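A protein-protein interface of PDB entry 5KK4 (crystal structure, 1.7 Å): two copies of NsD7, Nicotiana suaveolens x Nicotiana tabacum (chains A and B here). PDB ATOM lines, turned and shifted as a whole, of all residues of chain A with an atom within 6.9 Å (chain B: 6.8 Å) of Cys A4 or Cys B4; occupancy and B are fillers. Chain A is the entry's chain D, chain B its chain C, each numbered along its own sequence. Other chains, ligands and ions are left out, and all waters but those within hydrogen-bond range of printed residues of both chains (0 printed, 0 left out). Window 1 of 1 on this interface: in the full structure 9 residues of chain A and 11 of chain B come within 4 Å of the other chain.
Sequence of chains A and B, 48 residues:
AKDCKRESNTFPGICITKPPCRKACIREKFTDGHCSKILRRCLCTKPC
N of Lys B5 sits at hydrogen-bond distance from O of Lys A5 (2.9 Å). The side-chain amino group (NZ) of Lys A46 is in salt-bridge range of the chain-end carboxylate (O) of Cys B48 (3.2 Å). The chain-end carboxylate (O) of Cys A48 is in salt-bridge range of the side-chain amino group (NZ) of Lys B46 (3.3 Å). SG of Cys B48 sits at hydrogen-bond distance from NE of Arg A6 (3.4 Å).
The side-chain sulfur of Cys B48 forms a disulfide with the side-chain sulfur of Cys B4 (2.0 Å). N of Cys A44 lies within hydrogen-bond range of O of Arg A6, at 2.8 Å. The backbone carbonyl oxygen (O) of Lys B46 is in hydrogen-bond range of the backbone NH (N) of Cys B4. The backbone NH (N) of Cys B44 sits at hydrogen-bond distance from the backbone carbonyl oxygen (O) of Arg B6 (2.7 Å). The backbone carbonyl oxygen (O) of Lys A46 is in hydrogen-bond range of the backbone NH (N) of Cys A4. SG of Cys A4 forms a disulfide with SG of Cys A48 (2.0 Å).
CD of Arg B6 touches CB of Lys A2, 3.3 Å away. O of Asp A3 touches O of Lys B5, at 3.9 Å. CB of Cys B4 touches SG of Cys A4, 3.7 Å away. Lys B5 touches Cys A4 (O to CA, 3.4 Å). SG of Cys A4 touches CB of Arg B6, 3.9 Å away. CE2 of Phe B30 touches SG of Cys A4, 3.9 Å away. NE of Arg A6 touches O of Lys B2, 3.99 Å away. CB of Arg A6 touches O of Asp B3 (3.5 Å). CG of Arg A6 touches SG of Cys B4, at 3.96 Å. NE of Arg B6 touches CB of Cys A48, 3.9 Å away.
Cys A4 touches just these residues of chain B: Cys B4, Lys B5, Arg B6 and Phe B30. Thr A45 touches none of the printed residues of chain B. Of the printed residues of chain B, Lys A46 touches Cys B48 (3.2 Å). Of the printed residues of chain B, Cys A48 touches Arg B6 (3.9 Å) and Lys B46 (3.3 Å). Cys B4 touches four residues of chain A. The nearest residue of chain B that does not touch Cys A4 is Lys B46 (4.4 Å). The nearest residue of chain A that does not touch Cys B4 is Lys A46 (4.3 Å).
Hydrophobic or aromatic side chains of chain A that line the printed part of chain B: Phe A30. Along chain A the printed residues that touch a printed residue of chain B span positions 2 to 48. Hydrophobic or aromatic side chains of chain B that line the printed part of chain A: Phe B30. Among the printed residues, no Asp or Glu carboxylate lies within 4 Å of a Lys or Arg side-chain nitrogen of the other chain.
Asp A3 touches Lys B5, but with the chains exchanged Lys A5 does not touch Asp B3 (4.1 Å). Asp A3 touches Arg B6, and with the chains exchanged Arg A6 touches Asp B3. Cys A4 touches Lys B5, and with the chains exchanged Lys A5 touches Cys B4. Lys A5 touches its own counterpart, Lys B5. Positions printed for both chains: 2, 3, 4, 5, 6, 30, 44, 45, 46, 47 and 48.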
ATOM      1  N   LYS A   2      11.895   5.699 -11.550  1.00  0.00           N
ATOM      2  CA  LYS A   2      12.959   4.690 -11.269  1.00  0.00           C
ATOM      3  C   LYS A   2      14.356   5.323 -11.448  1.00  0.00           C
ATOM      4  O   LYS A   2      14.644   5.897 -12.504  1.00  0.00           O
ATOM      5  CB  LYS A   2      12.817   3.497 -12.207  1.00  0.00           C
ATOM      6  CG  LYS A   2      12.137   2.232 -11.679  1.00  0.00           C
ATOM      7  CD  LYS A   2      12.151   1.137 -12.764  1.00  0.00           C
ATOM      8  CE  LYS A   2      11.634  -0.214 -12.275  1.00  0.00           C
ATOM      9  NZ  LYS A   2      10.148  -0.346 -12.176  1.00  0.00           N
ATOM     10  N   ASP A   3      15.227   5.212 -10.440  1.00  0.00           N
ATOM     11  CA  ASP A   3      16.566   5.790 -10.503  1.00  0.00           C
ATOM     12  C   ASP A   3      17.589   4.728 -10.912  1.00  0.00           C
ATOM     13  O   ASP A   3      17.447   3.554 -10.560  1.00  0.00           O
ATOM     14  CB  ASP A   3      16.980   6.384  -9.154  1.00  0.00           C
ATOM     15  CG  ASP A   3      16.327   7.739  -8.854  1.00  0.00           C
ATOM     16  OD1 ASP A   3      15.839   8.414  -9.782  1.00  0.00           O
ATOM     17  OD2 ASP A   3      16.324   8.131  -7.667  1.00  0.00           O
ATOM     18  N   CYS A   4      18.629   5.151 -11.640  1.00  0.00           N
ATOM     19  CA  CYS A   4      19.820   4.339 -11.879  1.00  0.00           C
ATOM     20  C   CYS A   4      20.765   4.435 -10.688  1.00  0.00           C
ATOM     21  O   CYS A   4      20.839   5.462 -10.014  1.00  0.00           O
ATOM     22  CB  CYS A   4      20.581   4.797 -13.126  1.00  0.00           C
ATOM     23  SG  CYS A   4      20.197   3.914 -14.637  1.00  0.00           S
ATOM     24  N   LYS A   5      21.531   3.367 -10.469  1.00  0.00           N
ATOM     25  CA  LYS A   5      22.421   3.283  -9.320  1.00  0.00           C
ATOM     26  C   LYS A   5      23.768   2.708  -9.731  1.00  0.00           C
ATOM     27  O   LYS A   5      23.833   1.799 -10.563  1.00  0.00           O
ATOM     28  CB  LYS A   5      21.800   2.397  -8.261  1.00  0.00           C
ATOM     29  CG  LYS A   5      22.567   2.316  -6.968  1.00  0.00           C
ATOM     30  CD  LYS A   5      21.722   1.628  -5.926  1.00  0.00           C
ATOM     31  CE  LYS A   5      21.263   0.260  -6.426  1.00  0.00           C
ATOM     32  NZ  LYS A   5      20.542  -0.489  -5.389  1.00  0.00           N
ATOM     33  N   ARG A   6      24.846   3.241  -9.156  1.00  0.00           N
ATOM     34  CA  ARG A   6      26.125   2.563  -9.260  1.00  0.00           C
ATOM     35  C   ARG A   6      27.070   3.087  -8.193  1.00  0.00           C
ATOM     36  O   ARG A   6      26.911   4.193  -7.676  1.00  0.00           O
ATOM     37  CB  ARG A   6      26.744   2.721 -10.643  1.00  0.00           C
ATOM     38  CG  ARG A   6      27.290   4.059 -10.953  1.00  0.00           C
ATOM     39  CD  ARG A   6      28.677   3.883 -11.564  1.00  0.00           C
ATOM     40  NE  ARG A   6      29.126   5.082 -12.258  1.00  0.00           N
ATOM     41  CZ  ARG A   6      29.701   6.132 -11.677  1.00  0.00           C
ATOM     42  NH1 ARG A   6      29.913   6.165 -10.365  1.00  0.00           N
ATOM     43  NH2 ARG A   6      30.066   7.163 -12.422  1.00  0.00           N
ATOM     44  N   PHE A  30      25.683  12.565 -10.297  1.00  0.00           N
ATOM     45  CA  PHE A  30      24.463  11.928  -9.850  1.00  0.00           C
ATOM     46  C   PHE A  30      23.680  12.947  -9.033  1.00  0.00           C
ATOM     47  O   PHE A  30      24.107  14.095  -8.834  1.00  0.00           O
ATOM     48  CB  PHE A  30      24.780  10.656  -9.056  1.00  0.00           C
ATOM     49  CG  PHE A  30      25.332   9.556  -9.907  1.00  0.00           C
ATOM     50  CD1 PHE A  30      26.646   9.597 -10.340  1.00  0.00           C
ATOM     51  CD2 PHE A  30      24.535   8.484 -10.282  1.00  0.00           C
ATOM     52  CE1 PHE A  30      27.157   8.585 -11.138  1.00  0.00           C
ATOM     53  CE2 PHE A  30      25.033   7.471 -11.073  1.00  0.00           C
ATOM     54  CZ  PHE A  30      26.348   7.514 -11.503  1.00  0.00           C
ATOM     55  N   CYS A  44      25.676   5.737  -5.647  1.00  0.00           N
ATOM     56  CA  CYS A  44      25.151   6.950  -6.252  1.00  0.00           C
ATOM     57  C   CYS A  44      23.893   6.604  -7.031  1.00  0.00           C
ATOM     58  O   CYS A  44      23.771   5.509  -7.580  1.00  0.00           O
ATOM     59  CB  CYS A  44      26.184   7.581  -7.181  1.00  0.00           C
ATOM     60  SG  CYS A  44      27.769   7.944  -6.388  1.00  0.00           S
ATOM     61  N   THR A  45      22.942   7.536  -7.044  1.00  0.00           N
ATOM     62  CA  THR A  45      21.688   7.342  -7.753  1.00  0.00           C
ATOM     63  C   THR A  45      21.361   8.602  -8.550  1.00  0.00           C
ATOM     64  O   THR A  45      21.772   9.711  -8.183  1.00  0.00           O
ATOM     65  CB  THR A  45      20.518   7.034  -6.795  1.00  0.00           C
ATOM     66  OG1 THR A  45      20.435   8.050  -5.789  1.00  0.00           O
ATOM     67  CG2 THR A  45      20.671   5.650  -6.125  1.00  0.00           C
ATOM     68  N   LYS A  46      20.621   8.421  -9.641  1.00  0.00           N
ATOM     69  CA  LYS A  46      20.186   9.539 -10.478  1.00  0.00           C
ATOM     70  C   LYS A  46      19.075   9.056 -11.401  1.00  0.00           C
ATOM     71  O   LYS A  46      19.010   7.866 -11.738  1.00  0.00           O
ATOM     72  CB  LYS A  46      21.346  10.104 -11.304  1.00  0.00           C
ATOM     73  CG  LYS A  46      21.768   9.210 -12.467  1.00  0.00           C
ATOM     74  CD  LYS A  46      22.895   9.829 -13.248  1.00  0.00           C
ATOM     75  CE  LYS A  46      23.485   8.819 -14.207  1.00  0.00           C
ATOM     76  NZ  LYS A  46      24.531   9.418 -15.077  1.00  0.00           N
ATOM     77  N   PRO A  47      18.181   9.952 -11.820  1.00  0.00           N
ATOM     78  CA  PRO A  47      17.201   9.584 -12.848  1.00  0.00           C
ATOM     79  C   PRO A  47      17.902   9.079 -14.095  1.00  0.00           C
ATOM     80  O   PRO A  47      18.882   9.671 -14.553  1.00  0.00           O
ATOM     81  CB  PRO A  47      16.461  10.899 -13.119  1.00  0.00           C
ATOM     82  CG  PRO A  47      16.692  11.741 -11.931  1.00  0.00           C
ATOM     83  CD  PRO A  47      18.063  11.369 -11.434  1.00  0.00           C
ATOM     84  N   CYS A  48      17.382   7.983 -14.644  1.00  0.00           N
ATOM     85  CA  CYS A  48      17.993   7.308 -15.784  1.00  0.00           C
ATOM     86  C   CYS A  48      17.197   7.462 -17.075  1.00  0.00           C
ATOM     87  O   CYS A  48      17.651   7.053 -18.149  1.00  0.00           O
ATOM     88  CB  CYS A  48      18.168   5.826 -15.480  1.00  0.00           C
ATOM     89  SG  CYS A  48      19.808   5.413 -15.892  1.00  0.00           S
ATOM     90  OXT CYS A  48      16.086   7.994 -17.089  1.00  0.00           O
ATOM     91  N   LYS B   2      32.296   1.740 -14.829  1.00  0.00           N
ATOM     92  CA  LYS B   2      31.206   0.823 -14.398  1.00  0.00           C
ATOM     93  C   LYS B   2      29.824   1.255 -14.870  1.00  0.00           C
ATOM     94  O   LYS B   2      29.594   2.423 -15.190  1.00  0.00           O
ATOM     95  CB  LYS B   2      31.174   0.703 -12.883  1.00  0.00           C
ATOM     96  CG  LYS B   2      30.885  -0.709 -12.429  1.00  0.00           C
ATOM     97  CD  LYS B   2      32.102  -1.352 -11.778  1.00  0.00           C
ATOM     98  CE  LYS B   2      32.045  -1.280 -10.260  1.00  0.00           C
ATOM     99  NZ  LYS B   2      31.369  -0.050  -9.738  1.00  0.00           N
ATOM    100  N   ASP B   3      28.898   0.300 -14.875  1.00  0.00           N
ATOM    101  CA  ASP B   3      27.573   0.504 -15.433  1.00  0.00           C
ATOM    102  C   ASP B   3      26.562   0.850 -14.349  1.00  0.00           C
ATOM    103  O   ASP B   3      26.629   0.337 -13.224  1.00  0.00           O
ATOM    104  CB  ASP B   3      27.105  -0.737 -16.191  1.00  0.00           C
ATOM    105  CG  ASP B   3      27.711  -0.831 -17.582  1.00  0.00           C
ATOM    106  OD1 ASP B   3      28.735  -0.158 -17.832  1.00  0.00           O
ATOM    107  OD2 ASP B   3      27.167  -1.574 -18.426  1.00  0.00           O
ATOM    108  N   CYS B   4      25.645   1.745 -14.700  1.00  0.00           N
ATOM    109  CA  CYS B   4      24.450   2.014 -13.917  1.00  0.00           C
ATOM    110  C   CYS B   4      23.455   0.868 -14.047  1.00  0.00           C
ATOM    111  O   CYS B   4      23.371   0.208 -15.089  1.00  0.00           O
ATOM    112  CB  CYS B   4      23.790   3.303 -14.393  1.00  0.00           C
ATOM    113  SG  CYS B   4      24.655   4.749 -13.832  1.00  0.00           S
ATOM    114  N   LYS B   5      22.661   0.672 -12.995  1.00  0.00           N
ATOM    115  CA  LYS B   5      21.682  -0.405 -12.931  1.00  0.00           C
ATOM    116  C   LYS B   5      20.319   0.135 -12.519  1.00  0.00           C
ATOM    117  O   LYS B   5      20.214   1.002 -11.641  1.00  0.00           O
ATOM    118  CB  LYS B   5      22.143  -1.478 -11.944  1.00  0.00           C
ATOM    119  CG  LYS B   5      21.250  -2.664 -11.860  1.00  0.00           C
ATOM    120  CD  LYS B   5      21.963  -3.798 -11.148  1.00  0.00           C
ATOM    121  CE  LYS B   5      22.306  -3.441  -9.697  1.00  0.00           C
ATOM    122  NZ  LYS B   5      23.166  -4.484  -9.075  1.00  0.00           N
ATOM    123  N   ARG B   6      19.273  -0.366 -13.171  1.00  0.00           N
ATOM    124  CA  ARG B   6      17.908   0.025 -12.858  1.00  0.00           C
ATOM    125  C   ARG B   6      16.970  -1.114 -13.240  1.00  0.00           C
ATOM    126  O   ARG B   6      17.173  -1.775 -14.260  1.00  0.00           O
ATOM    127  CB  ARG B   6      17.488   1.291 -13.609  1.00  0.00           C
ATOM    128  CG  ARG B   6      15.991   1.338 -13.735  1.00  0.00           C
ATOM    129  CD  ARG B   6      15.387   2.641 -14.040  1.00  0.00           C
ATOM    130  NE  ARG B   6      15.391   3.110 -15.414  1.00  0.00           N
ATOM    131  CZ  ARG B   6      14.837   2.478 -16.442  1.00  0.00           C
ATOM    132  NH1 ARG B   6      14.285   1.271 -16.309  1.00  0.00           N
ATOM    133  NH2 ARG B   6      14.875   3.052 -17.635  1.00  0.00           N
ATOM    134  N   PHE B  30      19.026   0.403 -22.635  1.00  0.00           N
ATOM    135  CA  PHE B  30      20.159  -0.079 -21.872  1.00  0.00           C
ATOM    136  C   PHE B  30      20.943  -1.061 -22.738  1.00  0.00           C
ATOM    137  O   PHE B  30      20.516  -1.431 -23.833  1.00  0.00           O
ATOM    138  CB  PHE B  30      19.673  -0.743 -20.581  1.00  0.00           C
ATOM    139  CG  PHE B  30      19.105   0.219 -19.581  1.00  0.00           C
ATOM    140  CD1 PHE B  30      17.821   0.731 -19.728  1.00  0.00           C
ATOM    141  CD2 PHE B  30      19.858   0.621 -18.487  1.00  0.00           C
ATOM    142  CE1 PHE B  30      17.305   1.621 -18.810  1.00  0.00           C
ATOM    143  CE2 PHE B  30      19.341   1.517 -17.559  1.00  0.00           C
ATOM    144  CZ  PHE B  30      18.064   2.011 -17.718  1.00  0.00           C
ATOM    145  N   CYS B  44      18.302  -3.880 -15.580  1.00  0.00           N
ATOM    146  CA  CYS B  44      18.990  -3.380 -16.757  1.00  0.00           C
ATOM    147  C   CYS B  44      20.279  -2.674 -16.364  1.00  0.00           C
ATOM    148  O   CYS B  44      20.354  -2.015 -15.324  1.00  0.00           O
ATOM    149  CB  CYS B  44      18.085  -2.407 -17.498  1.00  0.00           C
ATOM    150  SG  CYS B  44      16.478  -3.141 -17.966  1.00  0.00           S
ATOM    151  N   THR B  45      21.291  -2.795 -17.220  1.00  0.00           N
ATOM    152  CA  THR B  45      22.554  -2.111 -16.993  1.00  0.00           C
ATOM    153  C   THR B  45      22.957  -1.331 -18.235  1.00  0.00           C
ATOM    154  O   THR B  45      22.669  -1.751 -19.365  1.00  0.00           O
ATOM    155  CB  THR B  45      23.654  -3.129 -16.616  1.00  0.00           C
ATOM    156  OG1 THR B  45      23.743  -4.149 -17.621  1.00  0.00           O
ATOM    157  CG2 THR B  45      23.325  -3.811 -15.301  1.00  0.00           C
ATOM    158  N   LYS B  46      23.597  -0.177 -18.033  1.00  0.00           N
ATOM    159  CA  LYS B  46      24.151   0.583 -19.145  1.00  0.00           C
ATOM    160  C   LYS B  46      25.257   1.492 -18.626  1.00  0.00           C
ATOM    161  O   LYS B  46      25.335   1.766 -17.421  1.00  0.00           O
ATOM    162  CB  LYS B  46      23.074   1.426 -19.846  1.00  0.00           C
ATOM    163  CG  LYS B  46      22.581   2.627 -19.014  1.00  0.00           C
ATOM    164  CD  LYS B  46      21.488   3.397 -19.737  1.00  0.00           C
ATOM    165  CE  LYS B  46      21.028   4.604 -18.930  1.00  0.00           C
ATOM    166  NZ  LYS B  46      20.036   5.446 -19.674  1.00  0.00           N
ATOM    167  N   PRO B  47      26.122   1.976 -19.519  1.00  0.00           N
ATOM    168  CA  PRO B  47      27.110   2.993 -19.143  1.00  0.00           C
ATOM    169  C   PRO B  47      26.448   4.222 -18.553  1.00  0.00           C
ATOM    170  O   PRO B  47      25.398   4.671 -19.021  1.00  0.00           O
ATOM    171  CB  PRO B  47      27.801   3.317 -20.473  1.00  0.00           C
ATOM    172  CG  PRO B  47      27.605   2.119 -21.307  1.00  0.00           C
ATOM    173  CD  PRO B  47      26.292   1.521 -20.908  1.00  0.00           C
ATOM    174  N   CYS B  48      27.079   4.768 -17.518  1.00  0.00           N
ATOM    175  CA  CYS B  48      26.569   5.951 -16.837  1.00  0.00           C
ATOM    176  C   CYS B  48      27.078   7.217 -17.507  1.00  0.00           C
ATOM    177  O   CYS B  48      26.486   8.288 -17.367  1.00  0.00           O
ATOM    178  CB  CYS B  48      26.986   5.945 -15.370  1.00  0.00           C
ATOM    179  SG  CYS B  48      26.564   4.462 -14.455  1.00  0.00           S
ATOM    180  OXT CYS B  48      28.097   7.194 -18.196  1.00  0.00           O
